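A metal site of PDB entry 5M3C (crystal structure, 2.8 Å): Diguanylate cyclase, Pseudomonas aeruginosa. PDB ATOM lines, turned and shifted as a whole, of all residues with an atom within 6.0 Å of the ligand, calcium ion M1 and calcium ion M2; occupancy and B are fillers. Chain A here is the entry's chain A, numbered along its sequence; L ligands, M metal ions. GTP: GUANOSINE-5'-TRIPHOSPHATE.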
ATOM      1  N   LEU A   8     -37.269  21.450  36.339  1.00  0.00           N
ATOM      2  CA  LEU A   8     -37.235  22.376  35.223  1.00  0.00           C
ATOM      3  C   LEU A   8     -37.817  21.782  33.943  1.00  0.00           C
ATOM      4  O   LEU A   8     -38.631  22.413  33.259  1.00  0.00           O
ATOM      5  CB  LEU A   8     -35.805  22.853  34.970  1.00  0.00           C
ATOM      6  CG  LEU A   8     -35.558  23.650  33.680  1.00  0.00           C
ATOM      7  CD1 LEU A   8     -36.534  24.812  33.539  1.00  0.00           C
ATOM      8  CD2 LEU A   8     -34.120  24.144  33.642  1.00  0.00           C
ATOM      9  N   ASP A  41     -24.727  16.593  24.827  1.00  0.00           N
ATOM     10  CA  ASP A  41     -24.309  17.817  25.494  1.00  0.00           C
ATOM     11  C   ASP A  41     -24.433  18.969  24.505  1.00  0.00           C
ATOM     12  O   ASP A  41     -24.051  18.842  23.341  1.00  0.00           O
ATOM     13  CB  ASP A  41     -22.862  17.678  25.990  1.00  0.00           C
ATOM     14  CG  ASP A  41     -22.338  18.950  26.607  1.00  0.00           C
ATOM     15  OD1 ASP A  41     -22.077  19.913  25.865  1.00  0.00           O
ATOM     16  OD2 ASP A  41     -22.162  18.980  27.839  1.00  0.00           O
ATOM     17  N   LEU A  42     -24.970  20.090  24.965  1.00  0.00           N
ATOM     18  CA  LEU A  42     -25.258  21.215  24.098  1.00  0.00           C
ATOM     19  C   LEU A  42     -24.000  21.968  23.688  1.00  0.00           C
ATOM     20  O   LEU A  42     -23.061  22.110  24.474  1.00  0.00           O
ATOM     21  CB  LEU A  42     -26.245  22.185  24.774  1.00  0.00           C
ATOM     22  CG  LEU A  42     -27.593  21.584  25.175  1.00  0.00           C
ATOM     23  CD1 LEU A  42     -28.378  22.575  26.016  1.00  0.00           C
ATOM     24  CD2 LEU A  42     -28.401  21.156  23.959  1.00  0.00           C
ATOM     25  N   ASP A  43     -23.979  22.450  22.442  1.00  0.00           N
ATOM     26  CA  ASP A  43     -22.824  23.158  21.904  1.00  0.00           C
ATOM     27  C   ASP A  43     -22.782  24.605  22.377  1.00  0.00           C
ATOM     28  O   ASP A  43     -23.726  25.365  22.179  1.00  0.00           O
ATOM     29  CB  ASP A  43     -22.826  23.102  20.375  1.00  0.00           C
ATOM     30  CG  ASP A  43     -22.425  21.738  19.833  1.00  0.00           C
ATOM     31  OD1 ASP A  43     -21.907  20.914  20.604  1.00  0.00           O
ATOM     32  OD2 ASP A  43     -22.623  21.496  18.618  1.00  0.00           O
ATOM     33  N   ARG A  44     -21.664  24.959  22.999  1.00  0.00           N
ATOM     34  CA  ARG A  44     -21.412  26.317  23.496  1.00  0.00           C
ATOM     35  C   ARG A  44     -22.651  26.976  24.104  1.00  0.00           C
ATOM     36  O   ARG A  44     -23.244  27.869  23.509  1.00  0.00           O
ATOM     37  CB  ARG A  44     -20.830  27.175  22.367  1.00  0.00           C
ATOM     38  CG  ARG A  44     -19.446  26.730  21.939  1.00  0.00           C
ATOM     39  CD  ARG A  44     -19.084  27.229  20.542  1.00  0.00           C
ATOM     40  N   PHE A  45     -23.008  26.522  25.306  1.00  0.00           N
ATOM     41  CA  PHE A  45     -24.211  27.001  25.989  1.00  0.00           C
ATOM     42  C   PHE A  45     -23.924  28.158  26.959  1.00  0.00           C
ATOM     43  O   PHE A  45     -24.820  28.957  27.228  1.00  0.00           O
ATOM     44  CB  PHE A  45     -24.889  25.856  26.730  1.00  0.00           C
ATOM     45  CG  PHE A  45     -26.366  26.046  26.911  1.00  0.00           C
ATOM     46  CD1 PHE A  45     -27.193  26.154  25.807  1.00  0.00           C
ATOM     47  CD2 PHE A  45     -26.931  26.126  28.172  1.00  0.00           C
ATOM     48  CE1 PHE A  45     -28.548  26.336  25.948  1.00  0.00           C
ATOM     49  CE2 PHE A  45     -28.295  26.307  28.325  1.00  0.00           C
ATOM     50  CZ  PHE A  45     -29.102  26.409  27.210  1.00  0.00           C
ATOM     51  N   LYS A  46     -22.708  28.229  27.479  1.00  0.00           N
ATOM     52  CA  LYS A  46     -22.340  29.337  28.378  1.00  0.00           C
ATOM     53  C   LYS A  46     -22.522  30.663  27.660  1.00  0.00           C
ATOM     54  O   LYS A  46     -23.173  31.586  28.172  1.00  0.00           O
ATOM     55  CB  LYS A  46     -20.897  29.191  28.861  1.00  0.00           C
ATOM     56  N   HIS A  47     -21.969  30.759  26.453  1.00  0.00           N
ATOM     57  CA  HIS A  47     -22.073  31.958  25.617  1.00  0.00           C
ATOM     58  C   HIS A  47     -23.525  32.387  25.444  1.00  0.00           C
ATOM     59  O   HIS A  47     -23.813  33.577  25.296  1.00  0.00           O
ATOM     60  CB  HIS A  47     -21.451  31.716  24.246  1.00  0.00           C
ATOM     61  N   ASN A  49     -25.959  31.588  27.785  1.00  0.00           N
ATOM     62  CA  ASN A  49     -26.399  32.018  29.113  1.00  0.00           C
ATOM     63  C   ASN A  49     -25.924  33.439  29.417  1.00  0.00           C
ATOM     64  O   ASN A  49     -26.639  34.213  30.050  1.00  0.00           O
ATOM     65  CB  ASN A  49     -25.883  31.068  30.200  1.00  0.00           C
ATOM     66  CG  ASN A  49     -26.890  29.986  30.539  1.00  0.00           C
ATOM     67  OD1 ASN A  49     -27.809  29.701  29.769  1.00  0.00           O
ATOM     68  ND2 ASN A  49     -26.708  29.366  31.703  1.00  0.00           N
ATOM     69  N   GLY A  53     -28.913  35.385  28.906  1.00  0.00           N
ATOM     70  CA  GLY A  53     -29.348  35.297  30.300  1.00  0.00           C
ATOM     71  C   GLY A  53     -30.144  34.042  30.609  1.00  0.00           C
ATOM     72  O   GLY A  53     -30.821  33.493  29.734  1.00  0.00           O
ATOM     73  N   HIS A  54     -30.074  33.600  31.855  1.00  0.00           N
ATOM     74  CA  HIS A  54     -30.780  32.397  32.310  1.00  0.00           C
ATOM     75  C   HIS A  54     -32.227  32.302  31.805  1.00  0.00           C
ATOM     76  O   HIS A  54     -32.656  31.230  31.365  1.00  0.00           O
ATOM     77  CB  HIS A  54     -30.773  32.311  33.842  1.00  0.00           C
ATOM     78  CG  HIS A  54     -29.840  31.263  34.376  1.00  0.00           C
ATOM     79  ND1 HIS A  54     -30.284  30.156  35.051  1.00  0.00           N
ATOM     80  CD2 HIS A  54     -28.493  31.172  34.327  1.00  0.00           C
ATOM     81  CE1 HIS A  54     -29.247  29.414  35.406  1.00  0.00           C
ATOM     82  NE2 HIS A  54     -28.151  30.007  34.983  1.00  0.00           N
ATOM     83  N   PRO A  55     -32.999  33.399  31.901  1.00  0.00           N
ATOM     84  CA  PRO A  55     -34.366  33.394  31.397  1.00  0.00           C
ATOM     85  C   PRO A  55     -34.501  32.608  30.096  1.00  0.00           C
ATOM     86  O   PRO A  55     -35.321  31.700  30.004  1.00  0.00           O
ATOM     87  CB  PRO A  55     -34.650  34.883  31.162  1.00  0.00           C
ATOM     88  CG  PRO A  55     -33.691  35.624  32.046  1.00  0.00           C
ATOM     89  CD  PRO A  55     -32.675  34.659  32.592  1.00  0.00           C
ATOM     90  N   ILE A  56     -33.705  32.971  29.094  1.00  0.00           N
ATOM     91  CA  ILE A  56     -33.727  32.302  27.803  1.00  0.00           C
ATOM     92  C   ILE A  56     -33.231  30.867  27.937  1.00  0.00           C
ATOM     93  O   ILE A  56     -33.823  29.928  27.385  1.00  0.00           O
ATOM     94  CB  ILE A  56     -32.863  33.046  26.766  1.00  0.00           C
ATOM     95  CG1 ILE A  56     -33.344  34.488  26.598  1.00  0.00           C
ATOM     96  CG2 ILE A  56     -32.880  32.314  25.433  1.00  0.00           C
ATOM     97  CD1 ILE A  56     -34.760  34.620  26.064  1.00  0.00           C
ATOM     98  N   GLY A  57     -32.137  30.689  28.675  1.00  0.00           N
ATOM     99  CA  GLY A  57     -31.558  29.371  28.904  1.00  0.00           C
ATOM    100  C   GLY A  57     -32.563  28.364  29.418  1.00  0.00           C
ATOM    101  O   GLY A  57     -32.923  27.423  28.707  1.00  0.00           O
ATOM    102  N   ASP A  58     -33.026  28.556  30.653  1.00  0.00           N
ATOM    103  CA  ASP A  58     -33.974  27.637  31.276  1.00  0.00           C
ATOM    104  C   ASP A  58     -35.125  27.282  30.345  1.00  0.00           C
ATOM    105  O   ASP A  58     -35.674  26.182  30.418  1.00  0.00           O
ATOM    106  CB  ASP A  58     -34.523  28.240  32.588  1.00  0.00           C
ATOM    107  CG  ASP A  58     -33.525  28.183  33.721  1.00  0.00           C
ATOM    108  OD1 ASP A  58     -32.325  28.446  33.473  1.00  0.00           O
ATOM    109  OD2 ASP A  58     -33.927  27.895  34.859  1.00  0.00           O
ATOM    110  N   LEU A  61     -33.843  24.900  27.314  1.00  0.00           N
ATOM    111  CA  LEU A  61     -33.721  23.537  27.819  1.00  0.00           C
ATOM    112  C   LEU A  61     -35.073  22.823  27.789  1.00  0.00           C
ATOM    113  O   LEU A  61     -35.162  21.673  27.370  1.00  0.00           O
ATOM    114  CB  LEU A  61     -33.145  23.534  29.239  1.00  0.00           C
ATOM    115  CG  LEU A  61     -31.699  24.017  29.380  1.00  0.00           C
ATOM    116  CD1 LEU A  61     -31.319  24.159  30.842  1.00  0.00           C
ATOM    117  CD2 LEU A  61     -30.741  23.091  28.662  1.00  0.00           C
ATOM    118  N   ARG A  80     -32.507  14.254  31.873  1.00  0.00           N
ATOM    119  CA  ARG A  80     -31.530  15.319  32.064  1.00  0.00           C
ATOM    120  C   ARG A  80     -30.604  14.883  33.175  1.00  0.00           C
ATOM    121  O   ARG A  80     -31.050  14.547  34.269  1.00  0.00           O
ATOM    122  CB  ARG A  80     -32.213  16.642  32.443  1.00  0.00           C
ATOM    123  CG  ARG A  80     -31.371  17.876  32.124  1.00  0.00           C
ATOM    124  CD  ARG A  80     -32.067  19.177  32.519  1.00  0.00           C
ATOM    125  NE  ARG A  80     -31.572  19.709  33.792  1.00  0.00           N
ATOM    126  CZ  ARG A  80     -30.905  20.860  33.925  1.00  0.00           C
ATOM    127  NH1 ARG A  80     -30.510  21.261  35.126  1.00  0.00           N
ATOM    128  NH2 ARG A  80     -30.645  21.617  32.872  1.00  0.00           N
ATOM    129  N   GLY A  82     -28.277  16.641  34.576  1.00  0.00           N
ATOM    130  CA  GLY A  82     -27.736  17.797  35.278  1.00  0.00           C
ATOM    131  C   GLY A  82     -26.936  18.634  34.308  1.00  0.00           C
ATOM    132  O   GLY A  82     -26.319  18.107  33.378  1.00  0.00           O
ATOM    133  N   GLY A  83     -26.945  19.946  34.522  1.00  0.00           N
ATOM    134  CA  GLY A  83     -26.288  20.862  33.590  1.00  0.00           C
ATOM    135  C   GLY A  83     -26.997  20.845  32.254  1.00  0.00           C
ATOM    136  O   GLY A  83     -28.200  20.603  32.173  1.00  0.00           O
ATOM    137  N   ASP A  84     -26.252  21.104  31.184  1.00  0.00           N
ATOM    138  CA  ASP A  84     -26.825  21.134  29.840  1.00  0.00           C
ATOM    139  C   ASP A  84     -26.652  19.778  29.168  1.00  0.00           C
ATOM    140  O   ASP A  84     -26.240  19.713  28.001  1.00  0.00           O
ATOM    141  CB  ASP A  84     -26.158  22.211  28.999  1.00  0.00           C
ATOM    142  CG  ASP A  84     -24.702  21.910  28.711  1.00  0.00           C
ATOM    143  OD1 ASP A  84     -24.107  21.071  29.417  1.00  0.00           O
ATOM    144  OD2 ASP A  84     -24.142  22.517  27.774  1.00  0.00           O
ATOM    145  N   GLU A  85     -26.971  18.703  29.881  1.00  0.00           N
ATOM    146  CA  GLU A  85     -26.660  17.361  29.421  1.00  0.00           C
ATOM    147  C   GLU A  85     -27.854  16.415  29.519  1.00  0.00           C
ATOM    148  O   GLU A  85     -28.429  16.230  30.589  1.00  0.00           O
ATOM    149  CB  GLU A  85     -25.470  16.812  30.199  1.00  0.00           C
ATOM    150  CG  GLU A  85     -24.168  17.554  29.925  1.00  0.00           C
ATOM    151  CD  GLU A  85     -23.046  17.208  30.894  1.00  0.00           C
ATOM    152  OE1 GLU A  85     -23.275  16.410  31.826  1.00  0.00           O
ATOM    153  OE2 GLU A  85     -21.934  17.740  30.702  1.00  0.00           O
ATOM    154  N   LYS A 154     -16.937  16.781  20.412  1.00  0.00           N
ATOM    155  CA  LYS A 154     -16.402  18.109  20.701  1.00  0.00           C
ATOM    156  C   LYS A 154     -15.021  18.240  20.062  1.00  0.00           C
ATOM    157  O   LYS A 154     -14.686  19.270  19.471  1.00  0.00           O
ATOM    158  CB  LYS A 154     -16.260  18.325  22.206  1.00  0.00           C
ATOM    159  CG  LYS A 154     -17.574  18.303  22.972  1.00  0.00           C
ATOM    160  CD  LYS A 154     -18.517  19.393  22.485  1.00  0.00           C
ATOM    161  CE  LYS A 154     -19.660  19.589  23.462  1.00  0.00           C
ATOM    162  NZ  LYS A 154     -20.777  20.339  22.825  1.00  0.00           N
ATOM    163  N   ARG A 158     -17.775  20.256  15.951  1.00  0.00           N
ATOM    164  CA  ARG A 158     -18.938  20.137  16.829  1.00  0.00           C
ATOM    165  C   ARG A 158     -20.184  19.774  16.031  1.00  0.00           C
ATOM    166  O   ARG A 158     -20.102  19.491  14.834  1.00  0.00           O
ATOM    167  CB  ARG A 158     -19.159  21.436  17.607  1.00  0.00           C
ATOM    168  CG  ARG A 158     -18.373  21.508  18.897  1.00  0.00           C
ATOM    169  CD  ARG A 158     -18.539  22.850  19.593  1.00  0.00           C
ATOM    170  NE  ARG A 158     -17.850  22.896  20.876  1.00  0.00           N
ATOM    171  CZ  ARG A 158     -16.527  22.880  21.036  1.00  0.00           C
ATOM    172  NH1 ARG A 158     -16.002  22.924  22.250  1.00  0.00           N
ATOM    173  NH2 ARG A 158     -15.729  22.805  19.980  1.00  0.00           N
ATOM    174  N   ASP A 234     -11.763  27.078  25.354  1.00  0.00           N
ATOM    175  CA  ASP A 234     -12.433  26.386  26.457  1.00  0.00           C
ATOM    176  C   ASP A 234     -12.002  26.903  27.824  1.00  0.00           C
ATOM    177  O   ASP A 234     -12.832  27.087  28.717  1.00  0.00           O
ATOM    178  CB  ASP A 234     -12.186  24.876  26.354  1.00  0.00           C
ATOM    179  CG  ASP A 234     -12.854  24.269  25.132  1.00  0.00           C
ATOM    180  OD1 ASP A 234     -14.000  24.659  24.816  1.00  0.00           O
ATOM    181  OD2 ASP A 234     -12.230  23.398  24.480  1.00  0.00           O
HETATM  182  PG  GTP L   1     -19.039  23.204  25.052  1.00  0.00           P
HETATM  183  O1G GTP L   1     -19.040  23.246  23.542  1.00  0.00           O
HETATM  184  O2G GTP L   1     -20.050  22.231  25.624  1.00  0.00           O
HETATM  185  O3G GTP L   1     -17.660  23.114  25.665  1.00  0.00           O
HETATM  186  O3B GTP L   1     -19.587  24.657  25.493  1.00  0.00           O
HETATM  187  PB  GTP L   1     -20.382  24.889  26.870  1.00  0.00           P
HETATM  188  O1B GTP L   1     -20.401  26.369  27.166  1.00  0.00           O
HETATM  189  O2B GTP L   1     -21.691  24.146  26.802  1.00  0.00           O
HETATM  190  O3A GTP L   1     -19.440  24.177  27.965  1.00  0.00           O
HETATM  191  PA  GTP L   1     -20.083  23.508  29.272  1.00  0.00           P
HETATM  192  O1A GTP L   1     -19.043  23.487  30.357  1.00  0.00           O
HETATM  193  O2A GTP L   1     -20.806  22.243  28.885  1.00  0.00           O
HETATM  194  O5' GTP L   1     -21.180  24.599  29.660  1.00  0.00           O
HETATM  195  C5' GTP L   1     -22.192  24.270  30.596  1.00  0.00           C
HETATM  196  C4' GTP L   1     -23.088  25.489  30.693  1.00  0.00           C
HETATM  197  O4' GTP L   1     -24.457  25.113  30.796  1.00  0.00           O
HETATM  198  C3' GTP L   1     -22.722  26.308  31.917  1.00  0.00           C
HETATM  199  O3' GTP L   1     -22.443  27.660  31.536  1.00  0.00           O
HETATM  200  C2' GTP L   1     -23.958  26.232  32.791  1.00  0.00           C
HETATM  201  O2' GTP L   1     -24.206  27.441  33.502  1.00  0.00           O
HETATM  202  C1' GTP L   1     -25.058  25.942  31.784  1.00  0.00           C
HETATM  203  N9  GTP L   1     -26.193  25.323  32.493  1.00  0.00           N
HETATM  204  C8  GTP L   1     -26.187  24.184  33.214  1.00  0.00           C
HETATM  205  N7  GTP L   1     -27.416  23.953  33.739  1.00  0.00           N
HETATM  206  C5  GTP L   1     -28.229  24.967  33.357  1.00  0.00           C
HETATM  207  C6  GTP L   1     -29.636  25.353  33.557  1.00  0.00           C
HETATM  208  O6  GTP L   1     -30.399  24.635  34.231  1.00  0.00           O
HETATM  209  N1  GTP L   1     -30.074  26.491  32.988  1.00  0.00           N
HETATM  210  C2  GTP L   1     -29.264  27.280  32.243  1.00  0.00           C
HETATM  211  N2  GTP L   1     -29.773  28.412  31.698  1.00  0.00           N
HETATM  212  N3  GTP L   1     -27.964  26.988  32.021  1.00  0.00           N
HETATM  213  C4  GTP L   1     -27.408  25.863  32.540  1.00  0.00           C
HETATM  214 CA    CA M   1     -22.197  21.838  26.752  1.00  0.00          CA
HETATM  215 CA    CA M   2     -21.841  20.181  30.218  1.00  0.00          CA
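An oxygen (O1G) of the ligand is in salt-bridge range of the side-chain amino group (NZ) of Lys 154 (3.5 Å). The backbone NH (N) of Arg 44 is in hydrogen-bond range of an oxygen (O1G) of the ligand. NH2 of Arg 80 sits at hydrogen-bond distance from O6 of the ligand (3.3 Å). An oxygen (O1B) of the ligand is in hydrogen-bond range of the backbone NH (N) of Phe 45 (3.2 Å). ND2 of Asn 49 sits at hydrogen-bond distance from N3 of the ligand (2.7 Å). NE of Arg 158 is in salt-bridge range of O1G of the ligand, at 2.9 Å. OD1 of Asp 58 sits at hydrogen-bond distance from N1 of the ligand, 3.0 Å away. N of Lys 46 lies within hydrogen-bond range of O1B of the ligand (3.0 Å).
The guanidinium group (NH1) of Arg 158 is in salt-bridge range of the side-chain carboxylate (OD1) of Asp 234 (3.7 Å). The side-chain amino group (NZ) of Lys 154 sits close to the side-chain carboxylate (OD1) of Asp 41 (3.3 Å). The backbone carbonyl oxygen (O) of Leu 42 sits close to the side-chain amino group (NZ) of Lys 154 (3.3 Å). The guanidinium group (NH2) of Arg 80 lies within hydrogen-bond range of the backbone carbonyl oxygen (O) of Gly 83, at 2.7 Å. The side-chain carboxylate of Asp 43 is in salt-bridge range of the side-chain amino group of Lys 154, 2.6 Å away. OD1 of Asp 58 is in hydrogen-bond range of ND1 of His 54 (3.1 Å).
Residues that only touch the ligand: Leu 8, His 54, Gly 57, Leu 61 and Gly 83. Hydrophobic or aromatic side chains within 4 Å of the ligand: Leu 8, Phe 45, His 54 and Leu 61. 16 residues have an atom within 4 Å of the ligand: Leu 8, Asp 41, Leu 42, Arg 44, Phe 45, Lys 46, Asn 49, His 54, Gly 57, Asp 58, Leu 61, Arg 80, Gly 83, Asp 84, Lys 154 and Arg 158. Along chain A the residues within 4 Å of the ligand span positions 8 to 158.
The nearest printed residue that does not touch calcium ion M1 is Lys 154 (4.4 Å).
Of the 24 residues printed, 3 come within 4 Å of calcium ion M2.
Calcium ion M1 is bound by the side-chain carboxylate of Asp 41, the side-chain carboxylate of Asp 84, an oxygen (O2B) of the ligand, the backbone carbonyl oxygen of Leu 42, an oxygen (O2G) of the ligand and an oxygen (O2A) of the ligand. Calcium ion M1 has six donor atoms within binding distance. Slightly farther from calcium ion M1 lies the side-chain carboxylate (OD2) of Asp 41 (3.1 Å).
Calcium ion M2 is bound by the side-chain carboxylate of Glu 85 (2.5 Å), the side-chain carboxylate of Asp 84 (2.6 Å), an oxygen (O2A) of the ligand (2.7 Å) and the side-chain carboxylate of Asp 41 (2.7 Å).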
